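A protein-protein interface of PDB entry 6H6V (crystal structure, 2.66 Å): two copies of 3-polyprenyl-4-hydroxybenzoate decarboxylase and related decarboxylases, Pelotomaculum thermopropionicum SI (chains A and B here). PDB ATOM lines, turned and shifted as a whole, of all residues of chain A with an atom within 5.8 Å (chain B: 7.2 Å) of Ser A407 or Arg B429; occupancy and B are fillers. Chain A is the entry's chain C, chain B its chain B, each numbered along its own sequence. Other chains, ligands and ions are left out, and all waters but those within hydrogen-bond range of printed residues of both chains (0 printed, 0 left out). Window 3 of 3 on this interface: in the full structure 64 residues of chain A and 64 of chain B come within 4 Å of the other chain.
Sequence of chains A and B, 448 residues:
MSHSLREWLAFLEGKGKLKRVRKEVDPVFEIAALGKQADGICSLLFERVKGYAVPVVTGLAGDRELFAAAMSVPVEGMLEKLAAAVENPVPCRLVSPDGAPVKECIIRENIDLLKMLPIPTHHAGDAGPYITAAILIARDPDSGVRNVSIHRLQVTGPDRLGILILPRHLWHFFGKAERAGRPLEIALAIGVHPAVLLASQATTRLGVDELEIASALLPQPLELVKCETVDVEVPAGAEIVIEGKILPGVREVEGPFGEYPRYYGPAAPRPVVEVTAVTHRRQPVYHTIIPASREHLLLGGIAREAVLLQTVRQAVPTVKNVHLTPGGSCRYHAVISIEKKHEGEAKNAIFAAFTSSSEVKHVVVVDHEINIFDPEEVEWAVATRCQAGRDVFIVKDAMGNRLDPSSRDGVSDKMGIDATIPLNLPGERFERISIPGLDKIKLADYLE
OG of Ser A406 sits at hydrogen-bond distance from OD1 of Asp A404, at 2.5 Å. NZ of Lys A361 sits at hydrogen-bond distance from OG of Ser A406 (3.0 Å). The backbone carbonyl oxygen (O) of Asn A401 sits at hydrogen-bond distance from the side-chain hydroxyl (OG) of Ser A407. The side-chain amino group of Lys A361 is in salt-bridge range of the side-chain carboxylate of Asp A404 (2.9 Å). The side-chain hydroxyl of Ser A407 lies within hydrogen-bond range of the backbone NH of Gly A410. The side-chain hydroxyl of Ser A407 sits at hydrogen-bond distance from the backbone carbonyl oxygen of Asp A404 (3.1 Å).
Ser A407 touches just these residues of chain B: Gln B387 and Arg B429. Of chain A, only Tyr A263, Pro A405 and Ser A407 come within 4 Å of Arg B429. Of the printed residues of chain A, Phe B430 touches Tyr A263, Pro A405 and Ser A406. Of the printed residues of chain B, Lys A361 touches Cys B386 (2.8 Å) and Gln B387 (3.4 Å). The nearest printed residue of chain A that does not touch Gln B387 is Val A411 (4.4 Å).
Of the 13 printed residues of chain B, 6 touch a printed residue of chain A. Hydrophobic or aromatic side chains of chain B that line the printed part of chain A: Phe B430. Of the 14 printed residues of chain A, 8 touch a printed residue of chain B. Hydrophobic or aromatic side chains of chain A that line the printed part of chain B: Tyr A263 and Pro A405. Along chain A the printed residues that touch a printed residue of chain B span positions 263 to 412.
Tyr A263 touches Arg B429. CE1 of Tyr A263 touches O of Phe B430 (3.4 Å). Asp A404 touches Gln B387 (OD2 to OE1, 3.5 Å). Thr B384 touches Pro A405 (O to CG, 3.7 Å). CZ of Arg B429 touches O of Pro A405, at 3.4 Å. Pro A405 touches Phe B430. Ser A406 touches Thr B384 (CB to O, 3.4 Å). Cys B386 touches Ser A406. Ser A406 touches Phe B430 (N to CE1, 3.9 Å). OE1 of Gln B387 touches N of Ser A407, 3.8 Å away.
OD1 of Asp A404 sits close to O of Thr B384 (3.3 Å). The side-chain amide nitrogen of Gln B387 lies close to the guanidinium group of Arg A408 (3.4 Å). The side-chain hydroxyl (OG1) of Thr B384 lies within hydrogen-bond range of the side-chain hydroxyl (OH) of Tyr A263 (2.6 Å). The side-chain amino group of Lys A361 is in hydrogen-bond range of the side-chain amide oxygen of Gln B387 (3.4 Å). The side-chain hydroxyl of Ser A406 is in hydrogen-bond range of the side-chain amide oxygen of Gln B387, 2.9 Å away. The backbone carbonyl oxygen of Cys B386 is in hydrogen-bond range of the side-chain amino group of Lys A361 (2.8 Å). OE1 of Gln B387 lies within hydrogen-bond range of OG of Ser A412 (3.1 Å).
No position is printed for both chains. Of the 19 pairs that touch across the chains among the printed residues, none has its exchanged pair printed and touching as well.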
ATOM      1  N   TYR A 263      25.020  13.307  17.719  1.00  0.00           N
ATOM      2  CA  TYR A 263      25.250  13.471  19.182  1.00  0.00           C
ATOM      3  C   TYR A 263      26.524  14.277  19.416  1.00  0.00           C
ATOM      4  O   TYR A 263      27.338  14.437  18.515  1.00  0.00           O
ATOM      5  CB  TYR A 263      25.380  12.122  19.899  1.00  0.00           C
ATOM      6  CG  TYR A 263      24.148  11.251  19.790  1.00  0.00           C
ATOM      7  CD1 TYR A 263      23.051  11.443  20.623  1.00  0.00           C
ATOM      8  CD2 TYR A 263      24.068  10.239  18.851  1.00  0.00           C
ATOM      9  CE1 TYR A 263      21.916  10.640  20.525  1.00  0.00           C
ATOM     10  CE2 TYR A 263      22.943   9.439  18.740  1.00  0.00           C
ATOM     11  CZ  TYR A 263      21.873   9.639  19.583  1.00  0.00           C
ATOM     12  OH  TYR A 263      20.743   8.863  19.441  1.00  0.00           O
ATOM     13  N   LYS A 361      26.772  -2.332  12.839  1.00  0.00           N
ATOM     14  CA  LYS A 361      25.984  -2.796  13.973  1.00  0.00           C
ATOM     15  C   LYS A 361      24.776  -3.644  13.543  1.00  0.00           C
ATOM     16  O   LYS A 361      24.557  -4.713  14.080  1.00  0.00           O
ATOM     17  CB  LYS A 361      25.542  -1.564  14.729  1.00  0.00           C
ATOM     18  CG  LYS A 361      24.840  -1.816  16.036  1.00  0.00           C
ATOM     19  CD  LYS A 361      24.574  -0.488  16.721  1.00  0.00           C
ATOM     20  CE  LYS A 361      23.841  -0.682  18.023  1.00  0.00           C
ATOM     21  NZ  LYS A 361      23.566   0.667  18.609  1.00  0.00           N
ATOM     22  N   ASN A 401      31.498   0.984  18.881  1.00  0.00           N
ATOM     23  CA  ASN A 401      31.928   2.345  18.631  1.00  0.00           C
ATOM     24  C   ASN A 401      31.682   3.171  19.890  1.00  0.00           C
ATOM     25  O   ASN A 401      30.604   3.079  20.477  1.00  0.00           O
ATOM     26  CB  ASN A 401      31.070   2.879  17.501  1.00  0.00           C
ATOM     27  CG  ASN A 401      31.619   4.142  16.895  1.00  0.00           C
ATOM     28  OD1 ASN A 401      32.745   4.143  16.388  1.00  0.00           O
ATOM     29  ND2 ASN A 401      30.832   5.218  16.924  1.00  0.00           N
ATOM     30  N   ARG A 402      32.657   3.977  20.312  1.00  0.00           N
ATOM     31  CA  ARG A 402      32.507   4.740  21.560  1.00  0.00           C
ATOM     32  C   ARG A 402      31.440   5.820  21.481  1.00  0.00           C
ATOM     33  O   ARG A 402      30.770   6.108  22.474  1.00  0.00           O
ATOM     34  CB  ARG A 402      33.826   5.359  22.013  1.00  0.00           C
ATOM     35  CG  ARG A 402      34.759   4.348  22.635  1.00  0.00           C
ATOM     36  CD  ARG A 402      36.006   5.002  23.221  1.00  0.00           C
ATOM     37  NE  ARG A 402      36.850   3.991  23.863  1.00  0.00           N
ATOM     38  CZ  ARG A 402      36.606   3.421  25.047  1.00  0.00           C
ATOM     39  NH1 ARG A 402      35.551   3.766  25.786  1.00  0.00           N
ATOM     40  NH2 ARG A 402      37.440   2.504  25.521  1.00  0.00           N
ATOM     41  N   LEU A 403      31.267   6.400  20.292  1.00  0.00           N
ATOM     42  CA  LEU A 403      30.370   7.528  20.107  1.00  0.00           C
ATOM     43  C   LEU A 403      28.895   7.151  20.006  1.00  0.00           C
ATOM     44  O   LEU A 403      28.031   7.999  20.223  1.00  0.00           O
ATOM     45  CB  LEU A 403      30.816   8.359  18.892  1.00  0.00           C
ATOM     46  CG  LEU A 403      30.769   9.885  19.091  1.00  0.00           C
ATOM     47  CD1 LEU A 403      31.736  10.357  20.151  1.00  0.00           C
ATOM     48  CD2 LEU A 403      30.957  10.559  17.760  1.00  0.00           C
ATOM     49  N   ASP A 404      28.604   5.902  19.654  1.00  0.00           N
ATOM     50  CA  ASP A 404      27.254   5.329  19.789  1.00  0.00           C
ATOM     51  C   ASP A 404      26.932   5.328  21.290  1.00  0.00           C
ATOM     52  O   ASP A 404      27.549   4.593  22.064  1.00  0.00           O
ATOM     53  CB  ASP A 404      27.203   3.922  19.144  1.00  0.00           C
ATOM     54  CG  ASP A 404      26.029   3.048  19.606  1.00  0.00           C
ATOM     55  OD1 ASP A 404      25.002   3.566  20.097  1.00  0.00           O
ATOM     56  OD2 ASP A 404      26.147   1.794  19.443  1.00  0.00           O
ATOM     57  N   PRO A 405      25.976   6.172  21.711  1.00  0.00           N
ATOM     58  CA  PRO A 405      25.701   6.308  23.131  1.00  0.00           C
ATOM     59  C   PRO A 405      24.969   5.122  23.759  1.00  0.00           C
ATOM     60  O   PRO A 405      24.941   5.013  24.993  1.00  0.00           O
ATOM     61  CB  PRO A 405      24.838   7.556  23.178  1.00  0.00           C
ATOM     62  CG  PRO A 405      24.121   7.572  21.870  1.00  0.00           C
ATOM     63  CD  PRO A 405      25.055   6.964  20.881  1.00  0.00           C
ATOM     64  N   SER A 406      24.386   4.244  22.939  1.00  0.00           N
ATOM     65  CA  SER A 406      23.823   3.006  23.453  1.00  0.00           C
ATOM     66  C   SER A 406      24.899   1.990  23.824  1.00  0.00           C
ATOM     67  O   SER A 406      24.604   1.004  24.501  1.00  0.00           O
ATOM     68  CB  SER A 406      22.873   2.375  22.438  1.00  0.00           C
ATOM     69  OG  SER A 406      23.595   1.850  21.331  1.00  0.00           O
ATOM     70  N   SER A 407      26.126   2.193  23.362  1.00  0.00           N
ATOM     71  CA  SER A 407      27.184   1.229  23.663  1.00  0.00           C
ATOM     72  C   SER A 407      27.684   1.360  25.110  1.00  0.00           C
ATOM     73  O   SER A 407      27.599   2.420  25.723  1.00  0.00           O
ATOM     74  CB  SER A 407      28.338   1.334  22.663  1.00  0.00           C
ATOM     75  OG  SER A 407      29.316   2.250  23.104  1.00  0.00           O
ATOM     76  N   ARG A 408      28.188   0.239  25.616  1.00  0.00           N
ATOM     77  CA  ARG A 408      28.697   0.074  26.970  1.00  0.00           C
ATOM     78  C   ARG A 408      30.219   0.261  26.864  1.00  0.00           C
ATOM     79  O   ARG A 408      31.007  -0.708  26.906  1.00  0.00           O
ATOM     80  CB  ARG A 408      28.326  -1.330  27.502  1.00  0.00           C
ATOM     81  CG  ARG A 408      26.900  -1.515  28.039  1.00  0.00           C
ATOM     82  CD  ARG A 408      25.738  -1.657  27.028  1.00  0.00           C
ATOM     83  NE  ARG A 408      25.826  -2.618  25.893  1.00  0.00           N
ATOM     84  CZ  ARG A 408      26.285  -3.870  25.929  1.00  0.00           C
ATOM     85  NH1 ARG A 408      26.746  -4.419  27.054  1.00  0.00           N
ATOM     86  NH2 ARG A 408      26.293  -4.595  24.813  1.00  0.00           N
ATOM     87  N   ASP A 409      30.624   1.515  26.674  1.00  0.00           N
ATOM     88  CA  ASP A 409      32.038   1.886  26.639  1.00  0.00           C
ATOM     89  C   ASP A 409      32.702   1.312  25.374  1.00  0.00           C
ATOM     90  O   ASP A 409      33.779   0.712  25.428  1.00  0.00           O
ATOM     91  CB  ASP A 409      32.728   1.413  27.947  1.00  0.00           C
ATOM     92  CG  ASP A 409      33.996   2.191  28.292  1.00  0.00           C
ATOM     93  OD1 ASP A 409      34.121   3.389  27.959  1.00  0.00           O
ATOM     94  OD2 ASP A 409      34.891   1.585  28.927  1.00  0.00           O
ATOM     95  N   GLY A 410      32.036   1.466  24.230  1.00  0.00           N
ATOM     96  CA  GLY A 410      32.506   0.876  22.971  1.00  0.00           C
ATOM     97  C   GLY A 410      32.129  -0.581  22.695  1.00  0.00           C
ATOM     98  O   GLY A 410      32.312  -1.060  21.577  1.00  0.00           O
ATOM     99  N   VAL A 411      31.638  -1.304  23.703  1.00  0.00           N
ATOM    100  CA  VAL A 411      31.108  -2.658  23.524  1.00  0.00           C
ATOM    101  C   VAL A 411      29.663  -2.564  23.043  1.00  0.00           C
ATOM    102  O   VAL A 411      28.872  -1.817  23.598  1.00  0.00           O
ATOM    103  CB  VAL A 411      31.184  -3.452  24.841  1.00  0.00           C
ATOM    104  CG1 VAL A 411      30.522  -4.812  24.733  1.00  0.00           C
ATOM    105  CG2 VAL A 411      32.644  -3.623  25.245  1.00  0.00           C
ATOM    106  N   SER A 412      29.320  -3.328  22.014  1.00  0.00           N
ATOM    107  CA  SER A 412      28.017  -3.221  21.377  1.00  0.00           C
ATOM    108  C   SER A 412      27.516  -4.565  20.902  1.00  0.00           C
ATOM    109  O   SER A 412      28.281  -5.410  20.484  1.00  0.00           O
ATOM    110  CB  SER A 412      28.086  -2.256  20.194  1.00  0.00           C
ATOM    111  OG  SER A 412      26.837  -2.147  19.514  1.00  0.00           O
ATOM    112  N   THR B 384      21.220   4.153  16.972  1.00  0.00           N
ATOM    113  CA  THR B 384      21.961   4.761  18.066  1.00  0.00           C
ATOM    114  C   THR B 384      21.362   4.580  19.440  1.00  0.00           C
ATOM    115  O   THR B 384      21.998   4.962  20.414  1.00  0.00           O
ATOM    116  CB  THR B 384      22.093   6.267  17.834  1.00  0.00           C
ATOM    117  OG1 THR B 384      20.795   6.849  17.777  1.00  0.00           O
ATOM    118  CG2 THR B 384      22.834   6.530  16.541  1.00  0.00           C
ATOM    119  N   CYS B 386      19.368   1.498  20.150  1.00  0.00           N
ATOM    120  CA  CYS B 386      19.034   0.102  20.313  1.00  0.00           C
ATOM    121  C   CYS B 386      20.315  -0.713  20.455  1.00  0.00           C
ATOM    122  O   CYS B 386      21.299  -0.495  19.759  1.00  0.00           O
ATOM    123  CB  CYS B 386      18.172  -0.386  19.139  1.00  0.00           C
ATOM    124  SG  CYS B 386      18.096  -2.176  18.969  1.00  0.00           S
ATOM    125  N   GLN B 387      20.293  -1.633  21.405  1.00  0.00           N
ATOM    126  CA  GLN B 387      21.300  -2.654  21.553  1.00  0.00           C
ATOM    127  C   GLN B 387      20.528  -3.972  21.514  1.00  0.00           C
ATOM    128  O   GLN B 387      19.787  -4.285  22.436  1.00  0.00           O
ATOM    129  CB  GLN B 387      22.012  -2.456  22.890  1.00  0.00           C
ATOM    130  CG  GLN B 387      22.982  -1.294  22.871  1.00  0.00           C
ATOM    131  CD  GLN B 387      24.265  -1.627  22.153  1.00  0.00           C
ATOM    132  OE1 GLN B 387      24.837  -0.796  21.418  1.00  0.00           O
ATOM    133  NE2 GLN B 387      24.731  -2.856  22.352  1.00  0.00           N
ATOM    134  N   ILE B 421      15.373   5.751  24.823  1.00  0.00           N
ATOM    135  CA  ILE B 421      16.482   6.057  25.724  1.00  0.00           C
ATOM    136  C   ILE B 421      16.211   5.413  27.094  1.00  0.00           C
ATOM    137  O   ILE B 421      15.074   5.432  27.561  1.00  0.00           O
ATOM    138  CB  ILE B 421      16.582   7.592  25.908  1.00  0.00           C
ATOM    139  CG1 ILE B 421      16.953   8.266  24.596  1.00  0.00           C
ATOM    140  CG2 ILE B 421      17.602   7.991  26.954  1.00  0.00           C
ATOM    141  CD1 ILE B 421      16.462   9.706  24.526  1.00  0.00           C
ATOM    142  N   PRO B 422      17.236   4.850  27.745  1.00  0.00           N
ATOM    143  CA  PRO B 422      17.027   4.381  29.118  1.00  0.00           C
ATOM    144  C   PRO B 422      16.648   5.523  30.032  1.00  0.00           C
ATOM    145  O   PRO B 422      17.143   6.636  29.881  1.00  0.00           O
ATOM    146  CB  PRO B 422      18.388   3.828  29.521  1.00  0.00           C
ATOM    147  CG  PRO B 422      19.058   3.464  28.231  1.00  0.00           C
ATOM    148  CD  PRO B 422      18.541   4.432  27.221  1.00  0.00           C
ATOM    149  N   LEU B 425      19.110   8.514  33.464  1.00  0.00           N
ATOM    150  CA  LEU B 425      20.491   8.642  33.040  1.00  0.00           C
ATOM    151  C   LEU B 425      20.815  10.109  32.972  1.00  0.00           C
ATOM    152  O   LEU B 425      19.900  10.951  32.995  1.00  0.00           O
ATOM    153  CB  LEU B 425      20.733   8.026  31.669  1.00  0.00           C
ATOM    154  CG  LEU B 425      21.123   6.540  31.652  1.00  0.00           C
ATOM    155  CD1 LEU B 425      21.378   6.070  30.242  1.00  0.00           C
ATOM    156  CD2 LEU B 425      22.226   6.137  32.649  1.00  0.00           C
ATOM    157  N   PRO B 426      22.118  10.451  32.855  1.00  0.00           N
ATOM    158  CA  PRO B 426      22.491  11.827  32.477  1.00  0.00           C
ATOM    159  C   PRO B 426      21.813  12.229  31.136  1.00  0.00           C
ATOM    160  O   PRO B 426      21.973  11.538  30.104  1.00  0.00           O
ATOM    161  CB  PRO B 426      24.014  11.782  32.367  1.00  0.00           C
ATOM    162  CG  PRO B 426      24.410  10.316  32.404  1.00  0.00           C
ATOM    163  CD  PRO B 426      23.289   9.588  33.130  1.00  0.00           C
ATOM    164  N   GLY B 427      21.034  13.302  31.167  1.00  0.00           N
ATOM    165  CA  GLY B 427      20.280  13.719  29.992  1.00  0.00           C
ATOM    166  C   GLY B 427      21.081  14.323  28.831  1.00  0.00           C
ATOM    167  O   GLY B 427      20.481  14.658  27.854  1.00  0.00           O
ATOM    168  N   GLU B 428      22.413  14.390  28.946  1.00  0.00           N
ATOM    169  CA  GLU B 428      23.257  14.951  27.900  1.00  0.00           C
ATOM    170  C   GLU B 428      23.848  13.865  27.015  1.00  0.00           C
ATOM    171  O   GLU B 428      24.377  14.186  25.949  1.00  0.00           O
ATOM    172  CB  GLU B 428      24.369  15.872  28.425  1.00  0.00           C
ATOM    173  CG  GLU B 428      23.921  17.321  28.728  1.00  0.00           C
ATOM    174  CD  GLU B 428      23.446  17.530  30.182  1.00  0.00           C
ATOM    175  OE1 GLU B 428      24.175  17.142  31.131  1.00  0.00           O
ATOM    176  OE2 GLU B 428      22.320  18.057  30.381  1.00  0.00           O
ATOM    177  N   ARG B 429      23.681  12.605  27.411  1.00  0.00           N
ATOM    178  CA  ARG B 429      24.293  11.506  26.671  1.00  0.00           C
ATOM    179  C   ARG B 429      23.593  11.253  25.341  1.00  0.00           C
ATOM    180  O   ARG B 429      24.231  11.021  24.326  1.00  0.00           O
ATOM    181  CB  ARG B 429      24.266  10.236  27.523  1.00  0.00           C
ATOM    182  CG  ARG B 429      25.192   9.128  27.055  1.00  0.00           C
ATOM    183  CD  ARG B 429      24.718   7.825  27.697  1.00  0.00           C
ATOM    184  NE  ARG B 429      25.773   6.842  27.920  1.00  0.00           N
ATOM    185  CZ  ARG B 429      25.571   5.571  28.286  1.00  0.00           C
ATOM    186  NH1 ARG B 429      24.333   5.079  28.467  1.00  0.00           N
ATOM    187  NH2 ARG B 429      26.622   4.763  28.470  1.00  0.00           N
ATOM    188  N   PHE B 430      22.263  11.256  25.378  1.00  0.00           N
ATOM    189  CA  PHE B 430      21.444  11.068  24.176  1.00  0.00           C
ATOM    190  C   PHE B 430      20.900  12.383  23.631  1.00  0.00           C
ATOM    191  O   PHE B 430      20.025  12.382  22.772  1.00  0.00           O
ATOM    192  CB  PHE B 430      20.295  10.085  24.450  1.00  0.00           C
ATOM    193  CG  PHE B 430      20.756   8.673  24.679  1.00  0.00           C
ATOM    194  CD1 PHE B 430      20.878   7.799  23.626  1.00  0.00           C
ATOM    195  CD2 PHE B 430      21.055   8.215  25.963  1.00  0.00           C
ATOM    196  CE1 PHE B 430      21.300   6.494  23.833  1.00  0.00           C
ATOM    197  CE2 PHE B 430      21.482   6.926  26.172  1.00  0.00           C
ATOM    198  CZ  PHE B 430      21.616   6.061  25.104  1.00  0.00           C
ATOM    199  N   GLU B 431      21.402  13.517  24.102  1.00  0.00           N
ATOM    200  CA  GLU B 431      20.958  14.822  23.610  1.00  0.00           C
ATOM    201  C   GLU B 431      21.357  14.953  22.147  1.00  0.00           C
ATOM    202  O   GLU B 431      22.545  14.957  21.779  1.00  0.00           O
ATOM    203  CB  GLU B 431      21.511  15.995  24.414  1.00  0.00           C
ATOM    204  CG  GLU B 431      20.839  17.331  24.116  1.00  0.00           C
ATOM    205  CD  GLU B 431      21.710  18.553  24.469  1.00  0.00           C
ATOM    206  OE1 GLU B 431      22.351  18.529  25.567  1.00  0.00           O
ATOM    207  OE2 GLU B 431      21.754  19.519  23.637  1.00  0.00           O
ATOM    208  N   ARG B 432      20.321  15.031  21.317  1.00  0.00           N
ATOM    209  CA  ARG B 432      20.446  15.230  19.895  1.00  0.00           C
ATOM    210  C   ARG B 432      20.939  16.648  19.576  1.00  0.00           C
ATOM    211  O   ARG B 432      20.471  17.623  20.169  1.00  0.00           O
ATOM    212  CB  ARG B 432      19.082  15.009  19.297  1.00  0.00           C
ATOM    213  CG  ARG B 432      19.038  14.994  17.807  1.00  0.00           C
ATOM    214  CD  ARG B 432      17.602  14.816  17.380  1.00  0.00           C
ATOM    215  NE  ARG B 432      17.554  14.483  15.966  1.00  0.00           N
ATOM    216  CZ  ARG B 432      16.442  14.390  15.250  1.00  0.00           C
ATOM    217  NH1 ARG B 432      15.246  14.620  15.810  1.00  0.00           N
ATOM    218  NH2 ARG B 432      16.546  14.075  13.961  1.00  0.00           N
